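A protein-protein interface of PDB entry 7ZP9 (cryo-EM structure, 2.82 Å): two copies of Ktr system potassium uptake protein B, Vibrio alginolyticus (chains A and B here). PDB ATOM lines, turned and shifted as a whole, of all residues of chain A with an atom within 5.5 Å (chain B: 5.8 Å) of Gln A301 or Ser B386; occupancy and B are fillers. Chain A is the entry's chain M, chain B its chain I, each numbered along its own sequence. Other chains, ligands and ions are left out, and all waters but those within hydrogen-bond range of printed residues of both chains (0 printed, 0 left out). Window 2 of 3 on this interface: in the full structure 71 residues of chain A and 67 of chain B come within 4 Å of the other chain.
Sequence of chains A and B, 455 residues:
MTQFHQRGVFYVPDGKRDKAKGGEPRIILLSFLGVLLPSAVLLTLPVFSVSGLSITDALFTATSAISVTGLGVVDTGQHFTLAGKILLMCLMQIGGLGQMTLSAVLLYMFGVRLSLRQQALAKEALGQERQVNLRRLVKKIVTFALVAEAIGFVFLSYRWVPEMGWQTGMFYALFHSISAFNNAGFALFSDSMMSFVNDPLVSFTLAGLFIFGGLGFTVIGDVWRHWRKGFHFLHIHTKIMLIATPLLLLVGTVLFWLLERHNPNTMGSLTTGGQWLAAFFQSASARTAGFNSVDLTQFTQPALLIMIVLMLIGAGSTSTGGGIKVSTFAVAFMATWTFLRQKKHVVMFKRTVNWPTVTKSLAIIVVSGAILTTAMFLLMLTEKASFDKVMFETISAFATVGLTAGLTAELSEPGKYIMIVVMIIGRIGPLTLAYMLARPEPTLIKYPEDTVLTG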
ATOM      1  N   PHE A 299     -26.712  30.900 -19.738  1.00  0.00           N
ATOM      2  CA  PHE A 299     -26.260  29.497 -19.567  1.00  0.00           C
ATOM      3  C   PHE A 299     -27.173  28.824 -18.545  1.00  0.00           C
ATOM      4  O   PHE A 299     -27.626  29.510 -17.615  1.00  0.00           O
ATOM      5  CB  PHE A 299     -24.815  29.472 -19.068  1.00  0.00           C
ATOM      6  CG  PHE A 299     -23.805  28.831 -19.983  1.00  0.00           C
ATOM      7  CD1 PHE A 299     -23.770  29.140 -21.332  1.00  0.00           C
ATOM      8  CD2 PHE A 299     -22.880  27.928 -19.489  1.00  0.00           C
ATOM      9  CE1 PHE A 299     -22.835  28.550 -22.166  1.00  0.00           C
ATOM     10  CE2 PHE A 299     -21.944  27.340 -20.323  1.00  0.00           C
ATOM     11  CZ  PHE A 299     -21.925  27.651 -21.662  1.00  0.00           C
ATOM     12  N   THR A 300     -27.414  27.522 -18.689  1.00  0.00           N
ATOM     13  CA  THR A 300     -28.235  26.807 -17.682  1.00  0.00           C
ATOM     14  C   THR A 300     -27.478  26.773 -16.351  1.00  0.00           C
ATOM     15  O   THR A 300     -26.242  26.728 -16.384  1.00  0.00           O
ATOM     16  CB  THR A 300     -28.643  25.414 -18.173  1.00  0.00           C
ATOM     17  OG1 THR A 300     -27.483  24.582 -18.225  1.00  0.00           O
ATOM     18  CG2 THR A 300     -29.332  25.446 -19.521  1.00  0.00           C
ATOM     19  N   GLN A 301     -28.200  26.783 -15.231  1.00  0.00           N
ATOM     20  CA  GLN A 301     -27.557  26.818 -13.892  1.00  0.00           C
ATOM     21  C   GLN A 301     -26.647  25.599 -13.709  1.00  0.00           C
ATOM     22  O   GLN A 301     -25.541  25.778 -13.184  1.00  0.00           O
ATOM     23  CB  GLN A 301     -28.621  26.845 -12.801  1.00  0.00           C
ATOM     24  CG  GLN A 301     -29.618  27.985 -12.938  1.00  0.00           C
ATOM     25  CD  GLN A 301     -29.182  29.224 -12.198  1.00  0.00           C
ATOM     26  OE1 GLN A 301     -29.883  29.725 -11.323  1.00  0.00           O
ATOM     27  NE2 GLN A 301     -28.004  29.721 -12.534  1.00  0.00           N
ATOM     28  N   PRO A 302     -27.054  24.371 -14.090  1.00  0.00           N
ATOM     29  CA  PRO A 302     -26.170  23.221 -13.976  1.00  0.00           C
ATOM     30  C   PRO A 302     -24.875  23.434 -14.771  1.00  0.00           C
ATOM     31  O   PRO A 302     -23.889  22.825 -14.432  1.00  0.00           O
ATOM     32  CB  PRO A 302     -27.001  22.081 -14.569  1.00  0.00           C
ATOM     33  CG  PRO A 302     -28.427  22.514 -14.354  1.00  0.00           C
ATOM     34  CD  PRO A 302     -28.387  24.009 -14.573  1.00  0.00           C
ATOM     35  N   ALA A 303     -24.901  24.296 -15.788  1.00  0.00           N
ATOM     36  CA  ALA A 303     -23.681  24.590 -16.578  1.00  0.00           C
ATOM     37  C   ALA A 303     -22.843  25.651 -15.866  1.00  0.00           C
ATOM     38  O   ALA A 303     -21.617  25.591 -15.989  1.00  0.00           O
ATOM     39  CB  ALA A 303     -24.044  25.027 -17.965  1.00  0.00           C
ATOM     40  N   LEU A 304     -23.474  26.603 -15.181  1.00  0.00           N
ATOM     41  CA  LEU A 304     -22.685  27.557 -14.409  1.00  0.00           C
ATOM     42  C   LEU A 304     -21.949  26.871 -13.266  1.00  0.00           C
ATOM     43  O   LEU A 304     -20.801  27.213 -12.965  1.00  0.00           O
ATOM     44  CB  LEU A 304     -23.581  28.672 -13.872  1.00  0.00           C
ATOM     45  CG  LEU A 304     -24.176  29.636 -14.895  1.00  0.00           C
ATOM     46  CD1 LEU A 304     -25.134  30.598 -14.216  1.00  0.00           C
ATOM     47  CD2 LEU A 304     -23.075  30.395 -15.614  1.00  0.00           C
ATOM     48  N   LEU A 305     -22.599  25.909 -12.610  1.00  0.00           N
ATOM     49  CA  LEU A 305     -21.948  25.192 -11.518  1.00  0.00           C
ATOM     50  C   LEU A 305     -20.760  24.383 -12.021  1.00  0.00           C
ATOM     51  O   LEU A 305     -19.725  24.303 -11.349  1.00  0.00           O
ATOM     52  CB  LEU A 305     -22.954  24.289 -10.808  1.00  0.00           C
ATOM     53  CG  LEU A 305     -22.418  23.517  -9.603  1.00  0.00           C
ATOM     54  CD1 LEU A 305     -21.851  24.472  -8.567  1.00  0.00           C
ATOM     55  CD2 LEU A 305     -23.509  22.661  -8.997  1.00  0.00           C
ATOM     56  N   ILE A 306     -20.892  23.770 -13.198  1.00  0.00           N
ATOM     57  CA  ILE A 306     -19.771  23.045 -13.789  1.00  0.00           C
ATOM     58  C   ILE A 306     -18.625  24.000 -14.100  1.00  0.00           C
ATOM     59  O   ILE A 306     -17.457  23.699 -13.831  1.00  0.00           O
ATOM     60  CB  ILE A 306     -20.230  22.280 -15.043  1.00  0.00           C
ATOM     61  CG1 ILE A 306     -21.062  21.060 -14.649  1.00  0.00           C
ATOM     62  CG2 ILE A 306     -19.036  21.863 -15.887  1.00  0.00           C
ATOM     63  CD1 ILE A 306     -20.421  20.208 -13.574  1.00  0.00           C
ATOM     64  N   ASP A 388     -26.319  33.395  -7.593  1.00  0.00           N
ATOM     65  CA  ASP A 388     -25.596  32.735  -8.678  1.00  0.00           C
ATOM     66  C   ASP A 388     -24.784  33.737  -9.494  1.00  0.00           C
ATOM     67  O   ASP A 388     -23.669  33.437  -9.934  1.00  0.00           O
ATOM     68  CB  ASP A 388     -26.569  31.957  -9.567  1.00  0.00           C
ATOM     69  CG  ASP A 388     -27.587  32.846 -10.256  1.00  0.00           C
ATOM     70  OD1 ASP A 388     -27.583  34.071 -10.024  1.00  0.00           O
ATOM     71  OD2 ASP A 388     -28.398  32.312 -11.041  1.00  0.00           O
ATOM     72  N   MET B 380     -29.919  20.110  -9.314  1.00  0.00           N
ATOM     73  CA  MET B 380     -30.190  21.054 -10.389  1.00  0.00           C
ATOM     74  C   MET B 380     -30.552  20.328 -11.675  1.00  0.00           C
ATOM     75  O   MET B 380     -31.329  20.837 -12.489  1.00  0.00           O
ATOM     76  CB  MET B 380     -28.975  21.946 -10.602  1.00  0.00           C
ATOM     77  CG  MET B 380     -28.909  23.080  -9.626  1.00  0.00           C
ATOM     78  SD  MET B 380     -27.533  24.179  -9.936  1.00  0.00           S
ATOM     79  CE  MET B 380     -28.410  25.718  -9.767  1.00  0.00           C
ATOM     80  N   LYS B 384     -35.745  21.869 -11.183  1.00  0.00           N
ATOM     81  CA  LYS B 384     -35.505  23.160 -11.815  1.00  0.00           C
ATOM     82  C   LYS B 384     -35.776  24.263 -10.803  1.00  0.00           C
ATOM     83  O   LYS B 384     -36.936  24.547 -10.487  1.00  0.00           O
ATOM     84  CB  LYS B 384     -36.384  23.334 -13.053  1.00  0.00           C
ATOM     85  N   ALA B 385     -34.710  24.878 -10.300  1.00  0.00           N
ATOM     86  CA  ALA B 385     -34.828  25.941  -9.311  1.00  0.00           C
ATOM     87  C   ALA B 385     -33.569  26.794  -9.364  1.00  0.00           C
ATOM     88  O   ALA B 385     -32.564  26.417  -9.971  1.00  0.00           O
ATOM     89  CB  ALA B 385     -35.050  25.379  -7.904  1.00  0.00           C
ATOM     90  N   SER B 386     -33.639  27.953  -8.713  1.00  0.00           N
ATOM     91  CA  SER B 386     -32.497  28.849  -8.661  1.00  0.00           C
ATOM     92  C   SER B 386     -31.380  28.235  -7.820  1.00  0.00           C
ATOM     93  O   SER B 386     -31.583  27.278  -7.070  1.00  0.00           O
ATOM     94  CB  SER B 386     -32.902  30.206  -8.089  1.00  0.00           C
ATOM     95  OG  SER B 386     -32.932  30.167  -6.674  1.00  0.00           O
ATOM     96  N   PHE B 387     -30.179  28.799  -7.965  1.00  0.00           N
ATOM     97  CA  PHE B 387     -29.009  28.190  -7.340  1.00  0.00           C
ATOM     98  C   PHE B 387     -29.032  28.366  -5.826  1.00  0.00           C
ATOM     99  O   PHE B 387     -28.640  27.459  -5.084  1.00  0.00           O
ATOM    100  CB  PHE B 387     -27.726  28.768  -7.932  1.00  0.00           C
ATOM    101  CG  PHE B 387     -26.473  28.155  -7.369  1.00  0.00           C
ATOM    102  CD1 PHE B 387     -26.073  26.890  -7.767  1.00  0.00           C
ATOM    103  CD2 PHE B 387     -25.708  28.827  -6.445  1.00  0.00           C
ATOM    104  CE1 PHE B 387     -24.933  26.312  -7.259  1.00  0.00           C
ATOM    105  CE2 PHE B 387     -24.563  28.248  -5.933  1.00  0.00           C
ATOM    106  CZ  PHE B 387     -24.172  26.994  -6.338  1.00  0.00           C
ATOM    107  N   ASP B 388     -29.475  29.533  -5.350  1.00  0.00           N
ATOM    108  CA  ASP B 388     -29.488  29.784  -3.911  1.00  0.00           C
ATOM    109  C   ASP B 388     -30.439  28.838  -3.188  1.00  0.00           C
ATOM    110  O   ASP B 388     -30.131  28.357  -2.093  1.00  0.00           O
ATOM    111  CB  ASP B 388     -29.859  31.242  -3.631  1.00  0.00           C
ATOM    112  CG  ASP B 388     -31.226  31.619  -4.173  1.00  0.00           C
ATOM    113  OD1 ASP B 388     -31.867  30.779  -4.834  1.00  0.00           O
ATOM    114  OD2 ASP B 388     -31.659  32.765  -3.936  1.00  0.00           O
ATOM    115  N   LYS B 389     -31.602  28.566  -3.779  1.00  0.00           N
ATOM    116  CA  LYS B 389     -32.541  27.640  -3.157  1.00  0.00           C
ATOM    117  C   LYS B 389     -31.978  26.225  -3.107  1.00  0.00           C
ATOM    118  O   LYS B 389     -32.040  25.572  -2.058  1.00  0.00           O
ATOM    119  CB  LYS B 389     -33.868  27.657  -3.913  1.00  0.00           C
ATOM    120  CG  LYS B 389     -34.565  29.007  -3.912  1.00  0.00           C
ATOM    121  CD  LYS B 389     -35.041  29.393  -2.522  1.00  0.00           C
ATOM    122  CE  LYS B 389     -35.805  30.710  -2.551  1.00  0.00           C
ATOM    123  NZ  LYS B 389     -36.248  31.138  -1.198  1.00  0.00           N
ATOM    124  N   VAL B 390     -31.422  25.746  -4.220  1.00  0.00           N
ATOM    125  CA  VAL B 390     -30.849  24.405  -4.258  1.00  0.00           C
ATOM    126  C   VAL B 390     -29.665  24.297  -3.310  1.00  0.00           C
ATOM    127  O   VAL B 390     -29.535  23.312  -2.575  1.00  0.00           O
ATOM    128  CB  VAL B 390     -30.456  24.036  -5.700  1.00  0.00           C
ATOM    129  CG1 VAL B 390     -29.596  22.786  -5.711  1.00  0.00           C
ATOM    130  CG2 VAL B 390     -31.695  23.840  -6.553  1.00  0.00           C
ATOM    131  N   MET B 391     -28.784  25.299  -3.309  1.00  0.00           N
ATOM    132  CA  MET B 391     -27.644  25.274  -2.401  1.00  0.00           C
ATOM    133  C   MET B 391     -28.095  25.289  -0.948  1.00  0.00           C
ATOM    134  O   MET B 391     -27.557  24.548  -0.120  1.00  0.00           O
ATOM    135  CB  MET B 391     -26.713  26.452  -2.683  1.00  0.00           C
ATOM    136  CG  MET B 391     -25.602  26.600  -1.657  1.00  0.00           C
ATOM    137  SD  MET B 391     -24.342  27.802  -2.109  1.00  0.00           S
ATOM    138  CE  MET B 391     -22.891  27.060  -1.367  1.00  0.00           C
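Of chain B, only Met B380 (3.2 Å), Ser B386 (3.8 Å) and Phe B387 (3.5 Å) come within 4 Å of Gln A301.
Ser B386 touches one residue of chain A.
Printed residues of chain A within 4 Å of Met B380: Gln A301 (3.2 Å) and Pro A302 (3.8 Å).
Of the printed residues of chain B, Leu A305 touches Phe B387.
Printed residues of chain A within 4 Å of Phe B387: Gln A301 (3.5 Å), Leu A305 (3.8 Å) and Asp A388 (3.8 Å).
Ile A306 touches none of the printed residues of chain B.
The nearest residue of chain B that does not touch Gln A301 is Ala B385 (4.5 Å).
The nearest printed residue of chain A that does not touch Ser B386 is Asp A388 (5.8 Å).
Met B380 touches Gln A301 (CE to CB, 3.2 Å).
Gln A301 touches Ser B386 (OE1 to CA, 3.8 Å).
Pro A302 touches Met B380.
Leu A305 touches Phe B387 (CD1 to CE1, 3.8 Å).
CB of Phe B387 touches CB of Asp A388, at 3.8 Å.
Of the 9 printed residues of chain B, 3 touch a printed residue of chain A.
Hydrophobic or aromatic side chains of chain B within 4 Å of the printed part of chain A: Met B380 and Phe B387.
Of the 9 printed residues of chain A, 4 touch a printed residue of chain B.
Printed residues of chain A that touch a printed residue of chain B: Gln A301, Pro A302, Leu A305 and Asp A388.
Among the printed residues, no Asp or Glu carboxylate lies within 4 Å of a Lys or Arg side-chain nitrogen of the other chain.
Position printed for both chains: 388.
Of the 6 pairs that touch across the chains among the printed residues, none has its exchanged pair printed and touching as well.
The side-chain carboxylate of Asp A388 lies close to the side-chain amide oxygen of Gln A301.
The backbone NH (N) of Phe B387 is in hydrogen-bond range of the side-chain amide oxygen (OE1) of Gln A301 (3.5 Å).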
